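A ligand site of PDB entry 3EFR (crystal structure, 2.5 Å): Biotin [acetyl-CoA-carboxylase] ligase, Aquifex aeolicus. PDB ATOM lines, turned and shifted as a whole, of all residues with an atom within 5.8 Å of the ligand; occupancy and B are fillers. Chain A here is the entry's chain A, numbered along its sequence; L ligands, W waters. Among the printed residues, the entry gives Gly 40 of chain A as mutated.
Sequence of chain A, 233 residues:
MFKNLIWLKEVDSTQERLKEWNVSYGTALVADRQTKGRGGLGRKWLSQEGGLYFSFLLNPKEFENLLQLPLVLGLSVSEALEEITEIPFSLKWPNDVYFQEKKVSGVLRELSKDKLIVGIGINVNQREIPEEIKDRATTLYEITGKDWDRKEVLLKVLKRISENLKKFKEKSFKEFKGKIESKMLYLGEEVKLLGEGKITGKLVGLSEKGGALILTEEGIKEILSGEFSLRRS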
ATOM      1  N   ASP A  12      22.953 -22.689  -3.035  1.00  0.00           N
ATOM      2  CA  ASP A  12      21.736 -21.938  -3.342  1.00  0.00           C
ATOM      3  C   ASP A  12      21.516 -20.873  -2.274  1.00  0.00           C
ATOM      4  O   ASP A  12      21.243 -19.714  -2.593  1.00  0.00           O
ATOM      5  CB  ASP A  12      20.525 -22.874  -3.430  1.00  0.00           C
ATOM      6  CG  ASP A  12      20.414 -23.817  -2.253  1.00  0.00           C
ATOM      7  OD1 ASP A  12      19.410 -24.554  -2.177  1.00  0.00           O
ATOM      8  OD2 ASP A  12      21.327 -23.834  -1.388  1.00  0.00           O
ATOM      9  N   SER A  13      21.670 -21.278  -1.020  1.00  0.00           N
ATOM     10  CA  SER A  13      21.541 -20.359   0.106  1.00  0.00           C
ATOM     11  C   SER A  13      22.031 -21.036   1.382  1.00  0.00           C
ATOM     12  O   SER A  13      21.606 -22.147   1.712  1.00  0.00           O
ATOM     13  CB  SER A  13      20.091 -19.922   0.277  1.00  0.00           C
ATOM     14  OG  SER A  13      19.897 -19.277   1.524  1.00  0.00           O
ATOM     15  N   THR A  14      22.932 -20.374   2.097  1.00  0.00           N
ATOM     16  CA  THR A  14      23.413 -20.890   3.367  1.00  0.00           C
ATOM     17  C   THR A  14      22.251 -21.122   4.324  1.00  0.00           C
ATOM     18  O   THR A  14      22.321 -21.972   5.217  1.00  0.00           O
ATOM     19  CB  THR A  14      24.428 -19.938   4.030  1.00  0.00           C
ATOM     20  OG1 THR A  14      23.880 -18.614   4.080  1.00  0.00           O
ATOM     21  CG2 THR A  14      25.719 -19.916   3.231  1.00  0.00           C
ATOM     22  N   GLN A  15      21.173 -20.381   4.119  1.00  0.00           N
ATOM     23  CA  GLN A  15      19.959 -20.544   4.905  1.00  0.00           C
ATOM     24  C   GLN A  15      19.298 -21.877   4.594  1.00  0.00           C
ATOM     25  O   GLN A  15      18.864 -22.601   5.492  1.00  0.00           O
ATOM     26  CB  GLN A  15      18.978 -19.403   4.628  1.00  0.00           C
ATOM     27  CG  GLN A  15      19.384 -18.068   5.229  1.00  0.00           C
ATOM     28  CD  GLN A  15      19.148 -18.009   6.722  1.00  0.00           C
ATOM     29  OE1 GLN A  15      18.010 -17.870   7.173  1.00  0.00           O
ATOM     30  NE2 GLN A  15      20.222 -18.120   7.507  1.00  0.00           N
ATOM     31  N   GLN A  34      26.247 -17.293  -3.826  1.00  0.00           N
ATOM     32  CA  GLN A  34      24.895 -17.786  -3.558  1.00  0.00           C
ATOM     33  C   GLN A  34      23.997 -17.614  -4.787  1.00  0.00           C
ATOM     34  O   GLN A  34      23.685 -16.488  -5.176  1.00  0.00           O
ATOM     35  CB  GLN A  34      24.282 -17.076  -2.361  1.00  0.00           C
ATOM     36  CG  GLN A  34      24.766 -17.593  -1.009  1.00  0.00           C
ATOM     37  CD  GLN A  34      24.097 -16.894   0.152  1.00  0.00           C
ATOM     38  OE1 GLN A  34      23.931 -15.666   0.151  1.00  0.00           O
ATOM     39  NE2 GLN A  34      23.716 -17.659   1.166  1.00  0.00           N
ATOM     40  N   LYS A  36      20.845 -18.700  -5.114  1.00  0.00           N
ATOM     41  CA  LYS A  36      19.462 -18.443  -4.720  1.00  0.00           C
ATOM     42  C   LYS A  36      19.368 -17.749  -3.369  1.00  0.00           C
ATOM     43  O   LYS A  36      18.494 -18.062  -2.567  1.00  0.00           O
ATOM     44  CB  LYS A  36      18.662 -19.750  -4.678  1.00  0.00           C
ATOM     45  CG  LYS A  36      18.343 -20.365  -6.030  1.00  0.00           C
ATOM     46  CD  LYS A  36      19.560 -21.017  -6.668  1.00  0.00           C
ATOM     47  CE  LYS A  36      19.168 -21.965  -7.775  1.00  0.00           C
ATOM     48  NZ  LYS A  36      18.474 -23.175  -7.252  1.00  0.00           N
ATOM     49  N   GLY A  37      20.275 -16.802  -3.125  1.00  0.00           N
ATOM     50  CA  GLY A  37      20.253 -16.057  -1.870  1.00  0.00           C
ATOM     51  C   GLY A  37      18.917 -15.381  -1.662  1.00  0.00           C
ATOM     52  O   GLY A  37      18.202 -15.090  -2.619  1.00  0.00           O
ATOM     53  N   ARG A  38      18.560 -15.140  -0.400  1.00  0.00           N
ATOM     54  CA  ARG A  38      17.281 -14.515  -0.086  1.00  0.00           C
ATOM     55  C   ARG A  38      17.374 -13.537   1.082  1.00  0.00           C
ATOM     56  O   ARG A  38      18.116 -13.752   2.044  1.00  0.00           O
ATOM     57  CB  ARG A  38      16.205 -15.569   0.191  1.00  0.00           C
ATOM     58  CG  ARG A  38      16.527 -16.505   1.343  1.00  0.00           C
ATOM     59  CD  ARG A  38      15.307 -17.334   1.711  1.00  0.00           C
ATOM     60  NE  ARG A  38      15.623 -18.396   2.662  1.00  0.00           N
ATOM     61  CZ  ARG A  38      15.893 -19.650   2.319  1.00  0.00           C
ATOM     62  NH1 ARG A  38      16.167 -20.547   3.249  1.00  0.00           N
ATOM     63  NH2 ARG A  38      15.874 -20.003   1.049  1.00  0.00           N
ATOM     64  N   GLY A  39      16.610 -12.443   0.995  1.00  0.00           N
ATOM     65  CA  GLY A  39      16.587 -11.440   2.043  1.00  0.00           C
ATOM     66  C   GLY A  39      17.227 -10.138   1.616  1.00  0.00           C
ATOM     67  O   GLY A  39      17.980 -10.087   0.636  1.00  0.00           O
ATOM     68  N   GLY A  40      16.910  -9.061   2.334  1.00  0.00           N
ATOM     69  CA  GLY A  40      17.515  -7.765   2.093  1.00  0.00           C
ATOM     70  C   GLY A  40      17.454  -7.269   0.660  1.00  0.00           C
ATOM     71  O   GLY A  40      16.399  -7.235   0.045  1.00  0.00           O
ATOM     72  N   LEU A  41      18.621  -6.885   0.139  1.00  0.00           N
ATOM     73  CA  LEU A  41      18.708  -6.204  -1.145  1.00  0.00           C
ATOM     74  C   LEU A  41      18.560  -7.108  -2.370  1.00  0.00           C
ATOM     75  O   LEU A  41      18.845  -6.698  -3.485  1.00  0.00           O
ATOM     76  CB  LEU A  41      20.025  -5.419  -1.232  1.00  0.00           C
ATOM     77  CG  LEU A  41      20.190  -4.344  -0.146  1.00  0.00           C
ATOM     78  CD1 LEU A  41      21.635  -3.889  -0.048  1.00  0.00           C
ATOM     79  CD2 LEU A  41      19.264  -3.168  -0.409  1.00  0.00           C
ATOM     80  N   TRP A  45      22.339  -9.704  -6.106  1.00  0.00           N
ATOM     81  CA  TRP A  45      23.572  -9.180  -5.529  1.00  0.00           C
ATOM     82  C   TRP A  45      24.125 -10.082  -4.438  1.00  0.00           C
ATOM     83  O   TRP A  45      25.269  -9.931  -4.013  1.00  0.00           O
ATOM     84  CB  TRP A  45      23.345  -7.776  -4.976  1.00  0.00           C
ATOM     85  CG  TRP A  45      22.918  -7.742  -3.547  1.00  0.00           C
ATOM     86  CD1 TRP A  45      21.798  -8.322  -3.015  1.00  0.00           C
ATOM     87  CD2 TRP A  45      23.592  -7.100  -2.463  1.00  0.00           C
ATOM     88  NE1 TRP A  45      21.738  -8.071  -1.661  1.00  0.00           N
ATOM     89  CE2 TRP A  45      22.830  -7.331  -1.304  1.00  0.00           C
ATOM     90  CE3 TRP A  45      24.770  -6.353  -2.365  1.00  0.00           C
ATOM     91  CZ2 TRP A  45      23.209  -6.839  -0.056  1.00  0.00           C
ATOM     92  CZ3 TRP A  45      25.144  -5.863  -1.137  1.00  0.00           C
ATOM     93  CH2 TRP A  45      24.369  -6.102   0.006  1.00  0.00           C
ATOM     94  N   LEU A  46      23.304 -11.015  -3.969  1.00  0.00           N
ATOM     95  CA  LEU A  46      23.744 -11.999  -2.976  1.00  0.00           C
ATOM     96  C   LEU A  46      24.538 -13.102  -3.653  1.00  0.00           C
ATOM     97  O   LEU A  46      25.020 -14.033  -2.998  1.00  0.00           O
ATOM     98  CB  LEU A  46      22.548 -12.578  -2.218  1.00  0.00           C
ATOM     99  CG  LEU A  46      21.944 -11.703  -1.115  1.00  0.00           C
ATOM    100  CD1 LEU A  46      20.760 -12.413  -0.469  1.00  0.00           C
ATOM    101  CD2 LEU A  46      22.990 -11.343  -0.068  1.00  0.00           C
ATOM    102  N   LEU A  52      30.285 -11.216   2.148  1.00  0.00           N
ATOM    103  CA  LEU A  52      30.435 -12.223   3.195  1.00  0.00           C
ATOM    104  C   LEU A  52      29.077 -12.808   3.559  1.00  0.00           C
ATOM    105  O   LEU A  52      28.298 -12.209   4.292  1.00  0.00           O
ATOM    106  CB  LEU A  52      31.105 -11.614   4.430  1.00  0.00           C
ATOM    107  CG  LEU A  52      31.579 -12.591   5.507  1.00  0.00           C
ATOM    108  CD1 LEU A  52      32.470 -13.670   4.907  1.00  0.00           C
ATOM    109  CD2 LEU A  52      32.297 -11.862   6.633  1.00  0.00           C
ATOM    110  N   TYR A  53      28.792 -14.008   3.035  1.00  0.00           N
ATOM    111  CA  TYR A  53      27.503 -14.650   3.264  1.00  0.00           C
ATOM    112  C   TYR A  53      27.662 -15.893   4.129  1.00  0.00           C
ATOM    113  O   TYR A  53      28.371 -16.826   3.765  1.00  0.00           O
ATOM    114  CB  TYR A  53      26.858 -15.024   1.934  1.00  0.00           C
ATOM    115  CG  TYR A  53      27.070 -13.984   0.845  1.00  0.00           C
ATOM    116  CD1 TYR A  53      27.903 -14.234  -0.233  1.00  0.00           C
ATOM    117  CD2 TYR A  53      26.431 -12.743   0.907  1.00  0.00           C
ATOM    118  CE1 TYR A  53      28.098 -13.305  -1.221  1.00  0.00           C
ATOM    119  CE2 TYR A  53      26.628 -11.800  -0.083  1.00  0.00           C
ATOM    120  CZ  TYR A  53      27.464 -12.085  -1.147  1.00  0.00           C
ATOM    121  OH  TYR A  53      27.653 -11.147  -2.135  1.00  0.00           O
ATOM    122  N   PHE A  54      26.990 -15.911   5.272  1.00  0.00           N
ATOM    123  CA  PHE A  54      27.059 -17.059   6.169  1.00  0.00           C
ATOM    124  C   PHE A  54      25.800 -17.194   7.025  1.00  0.00           C
ATOM    125  O   PHE A  54      25.062 -16.237   7.197  1.00  0.00           O
ATOM    126  CB  PHE A  54      28.300 -16.972   7.066  1.00  0.00           C
ATOM    127  CG  PHE A  54      28.269 -15.840   8.048  1.00  0.00           C
ATOM    128  CD1 PHE A  54      27.856 -16.054   9.358  1.00  0.00           C
ATOM    129  CD2 PHE A  54      28.646 -14.567   7.669  1.00  0.00           C
ATOM    130  CE1 PHE A  54      27.820 -15.007  10.269  1.00  0.00           C
ATOM    131  CE2 PHE A  54      28.618 -13.514   8.577  1.00  0.00           C
ATOM    132  CZ  PHE A  54      28.208 -13.738   9.877  1.00  0.00           C
ATOM    133  N   SER A  55      25.584 -18.393   7.552  1.00  0.00           N
ATOM    134  CA  SER A  55      24.454 -18.660   8.423  1.00  0.00           C
ATOM    135  C   SER A  55      24.883 -19.563   9.586  1.00  0.00           C
ATOM    136  O   SER A  55      25.910 -20.230   9.515  1.00  0.00           O
ATOM    137  CB  SER A  55      23.317 -19.316   7.641  1.00  0.00           C
ATOM    138  OG  SER A  55      22.878 -18.484   6.573  1.00  0.00           O
ATOM    139  N   ASN A  95      17.294  -4.493  12.065  1.00  0.00           N
ATOM    140  CA  ASN A  95      18.348  -5.468  11.796  1.00  0.00           C
ATOM    141  C   ASN A  95      19.549  -4.955  10.993  1.00  0.00           C
ATOM    142  O   ASN A  95      20.694  -5.333  11.263  1.00  0.00           O
ATOM    143  CB  ASN A  95      17.756  -6.704  11.094  1.00  0.00           C
ATOM    144  CG  ASN A  95      16.988  -6.351   9.832  1.00  0.00           C
ATOM    145  OD1 ASN A  95      16.604  -5.196   9.623  1.00  0.00           O
ATOM    146  ND2 ASN A  95      16.754  -7.338   8.980  1.00  0.00           N
ATOM    147  N   ASP A  96      19.295  -4.101  10.001  1.00  0.00           N
ATOM    148  CA  ASP A  96      20.337  -3.674   9.070  1.00  0.00           C
ATOM    149  C   ASP A  96      21.464  -2.851   9.700  1.00  0.00           C
ATOM    150  O   ASP A  96      21.237  -2.058  10.616  1.00  0.00           O
ATOM    151  CB  ASP A  96      19.717  -2.895   7.907  1.00  0.00           C
ATOM    152  CG  ASP A  96      18.712  -3.716   7.123  1.00  0.00           C
ATOM    153  OD1 ASP A  96      18.766  -4.960   7.205  1.00  0.00           O
ATOM    154  OD2 ASP A  96      17.863  -3.106   6.441  1.00  0.00           O
ATOM    155  N   LYS A 103      23.269   0.804   3.169  1.00  0.00           N
ATOM    156  CA  LYS A 103      23.401  -0.408   3.975  1.00  0.00           C
ATOM    157  C   LYS A 103      24.703  -1.151   3.721  1.00  0.00           C
ATOM    158  O   LYS A 103      25.207  -1.172   2.593  1.00  0.00           O
ATOM    159  CB  LYS A 103      22.215  -1.357   3.748  1.00  0.00           C
ATOM    160  CG  LYS A 103      22.373  -2.712   4.420  1.00  0.00           C
ATOM    161  CD  LYS A 103      21.044  -3.404   4.654  1.00  0.00           C
ATOM    162  CE  LYS A 103      20.570  -4.173   3.431  1.00  0.00           C
ATOM    163  NZ  LYS A 103      19.416  -5.065   3.760  1.00  0.00           N
ATOM    164  N   SER A 105      25.243  -4.216   5.870  1.00  0.00           N
ATOM    165  CA  SER A 105      24.942  -5.562   6.332  1.00  0.00           C
ATOM    166  C   SER A 105      23.467  -5.745   6.697  1.00  0.00           C
ATOM    167  O   SER A 105      22.783  -4.784   7.043  1.00  0.00           O
ATOM    168  CB  SER A 105      25.819  -5.926   7.527  1.00  0.00           C
ATOM    169  OG  SER A 105      25.594  -7.257   7.949  1.00  0.00           O
ATOM    170  N   GLY A 106      22.996  -6.978   6.639  1.00  0.00           N
ATOM    171  CA  GLY A 106      21.622  -7.286   6.984  1.00  0.00           C
ATOM    172  C   GLY A 106      21.513  -8.591   7.736  1.00  0.00           C
ATOM    173  O   GLY A 106      22.210  -9.558   7.419  1.00  0.00           O
ATOM    174  N   VAL A 107      20.647  -8.622   8.752  1.00  0.00           N
ATOM    175  CA  VAL A 107      20.471  -9.818   9.560  1.00  0.00           C
ATOM    176  C   VAL A 107      19.123 -10.501   9.300  1.00  0.00           C
ATOM    177  O   VAL A 107      18.062  -9.897   9.480  1.00  0.00           O
ATOM    178  CB  VAL A 107      20.606  -9.507  11.065  1.00  0.00           C
ATOM    179  CG1 VAL A 107      20.242 -10.730  11.891  1.00  0.00           C
ATOM    180  CG2 VAL A 107      22.020  -9.045  11.387  1.00  0.00           C
ATOM    181  N   LEU A 108      19.182 -11.745   8.863  1.00  0.00           N
ATOM    182  CA  LEU A 108      17.978 -12.525   8.579  1.00  0.00           C
ATOM    183  C   LEU A 108      17.839 -13.669   9.568  1.00  0.00           C
ATOM    184  O   LEU A 108      18.830 -14.272   9.975  1.00  0.00           O
ATOM    185  CB  LEU A 108      18.033 -13.086   7.149  1.00  0.00           C
ATOM    186  CG  LEU A 108      16.907 -14.036   6.721  1.00  0.00           C
ATOM    187  CD1 LEU A 108      15.555 -13.326   6.721  1.00  0.00           C
ATOM    188  CD2 LEU A 108      17.200 -14.624   5.360  1.00  0.00           C
ATOM    189  N   GLY A 119      20.867 -15.755   9.140  1.00  0.00           N
ATOM    190  CA  GLY A 119      21.669 -15.462   7.964  1.00  0.00           C
ATOM    191  C   GLY A 119      22.157 -14.025   7.953  1.00  0.00           C
ATOM    192  O   GLY A 119      21.370 -13.099   8.141  1.00  0.00           O
ATOM    193  N   ILE A 120      23.456 -13.842   7.735  1.00  0.00           N
ATOM    194  CA  ILE A 120      24.048 -12.517   7.742  1.00  0.00           C
ATOM    195  C   ILE A 120      24.853 -12.254   6.475  1.00  0.00           C
ATOM    196  O   ILE A 120      25.708 -13.056   6.100  1.00  0.00           O
ATOM    197  CB  ILE A 120      24.938 -12.301   8.969  1.00  0.00           C
ATOM    198  CG1 ILE A 120      24.096 -12.243  10.238  1.00  0.00           C
ATOM    199  CG2 ILE A 120      25.763 -11.033   8.812  1.00  0.00           C
ATOM    200  CD1 ILE A 120      24.904 -12.022  11.495  1.00  0.00           C
ATOM    201  N   GLY A 121      24.570 -11.134   5.821  1.00  0.00           N
ATOM    202  CA  GLY A 121      25.320 -10.720   4.653  1.00  0.00           C
ATOM    203  C   GLY A 121      26.077  -9.430   4.904  1.00  0.00           C
ATOM    204  O   GLY A 121      25.490  -8.446   5.368  1.00  0.00           O
HETATM  205  C1  LIG L   1      19.270  -8.946   4.817  1.00  0.00           C
HETATM  206  O1  LIG L   1      18.898  -8.126   5.683  1.00  0.00           O
HETATM  207  O2  LIG L   1      19.810  -8.530   3.774  1.00  0.00           O
HETATM  208  C2  LIG L   1      19.044 -10.426   5.049  1.00  0.00           C
HETATM  209  C3  LIG L   1      20.369 -11.168   5.131  1.00  0.00           C
HETATM  210  C4  LIG L   1      21.074 -11.133   3.781  1.00  0.00           C
HETATM  211  C5  LIG L   1      21.221 -12.528   3.195  1.00  0.00           C
HETATM  212  C6  LIG L   1      22.051 -13.445   4.074  1.00  0.00           C
HETATM  213  S1  LIG L   1      23.527 -13.698   3.324  1.00  0.00           S
HETATM  214  C7  LIG L   1      23.614 -15.417   3.880  1.00  0.00           C
HETATM  215  C8  LIG L   1      22.242 -15.939   4.250  1.00  0.00           C
HETATM  216  N1  LIG L   1      21.676 -16.751   3.190  1.00  0.00           N
HETATM  217  C9  LIG L   1      20.633 -16.163   2.631  1.00  0.00           C
HETATM  218  O3  LIG L   1      19.883 -16.688   1.552  1.00  0.00           O
HETATM  219  N2  LIG L   1      20.367 -15.013   3.234  1.00  0.00           N
HETATM  220  C10 LIG L   1      21.302 -14.750   4.310  1.00  0.00           C
HETATM  221  O   HOH W   1      21.251  -8.613   1.240  1.00  0.00           O
HETATM  222  O   HOH W   2      16.002  -9.279   6.659  1.00  0.00           O
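The side-chain hydroxyl (OG) of Ser 13 lies within hydrogen-bond range of an oxygen (O3) of the ligand (2.6 Å). An oxygen (O3) of the ligand sits at hydrogen-bond distance from the backbone NH (N) of Arg 38. A nitrogen (N2) of the ligand sits at hydrogen-bond distance from the backbone carbonyl oxygen (O) of Arg 38, at 2.8 Å. The backbone NH (N) of Gly 40 lies close to an oxygen (O2) of the ligand, 3.3 Å away. NE2 of Gln 34 lies close to N1 of the ligand, at 3.0 Å. OG1 of Thr 14 lies within hydrogen-bond range of N1 of the ligand (3.0 Å). The side-chain amino group of Lys 103 lies within salt-bridge range of an oxygen (O2) of the ligand (3.5 Å). The backbone NH (N) of Gly 121 sits close to a sulfur (S1) of the ligand.
The side-chain hydroxyl of Ser 13 sits close to the backbone NH of Gln 15. N of Thr 14 lies close to NE2 of Gln 34 (3.0 Å). OG1 of Thr 14 lies within hydrogen-bond range of OG of Ser 55, 2.7 Å away. NE2 of Gln 15 lies close to N of Gly 119, at 2.9 Å. NZ of Lys 103 lies within salt-bridge range of OD1 of Asp 96, 3.5 Å away. The side-chain amide oxygen (OD1) of Asn 95 lies close to the side-chain carboxylate (OD1) of Asp 96 (3.3 Å). ND2 of Asn 95 sits at hydrogen-bond distance from O of Val 107, 2.9 Å away. The side-chain hydroxyl (OH) of Tyr 53 sits at hydrogen-bond distance from the backbone carbonyl oxygen (O) of Trp 45, at 3.3 Å.
The backbone carbonyl oxygen (O) of Ile 120 lies close to a sulfur (S1) of the ligand, 3.6 Å away. Merely in contact with the ligand: Gly 106 (3.1 Å), Gln 15 (3.3 Å), Gly 37 (3.5 Å), Ser 55 (3.5 Å), Asp 96 (3.5 Å), Leu 108 (3.5 Å), Val 107 (3.6 Å), Phe 54 (3.7 Å), Leu 46 (3.7 Å), Gly 119 (3.7 Å), Gly 39 (3.7 Å) and Tyr 53 (3.8 Å). Hydrophobic or aromatic side chains within 4 Å of the ligand: Leu 46, Tyr 53 and Leu 108. 20 residues have an atom within 4 Å of the ligand: Ser 13, Thr 14, Gln 15, Gln 34, Gly 37, Arg 38, Gly 39, Gly 40, Leu 46, Tyr 53, Phe 54, Ser 55, Asp 96, Lys 103, Gly 106, Val 107, Leu 108, Gly 119, Ile 120 and Gly 121. The nearest printed residue that does not touch the ligand is Asn 95 (4.01 Å).
Water W1 lies within hydrogen-bond range of an oxygen (O2) of the ligand, the indole nitrogen of Trp 45 and the backbone NH of Leu 41. Water W2 bridges ND2 of Asn 95 and O1 of the ligand.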
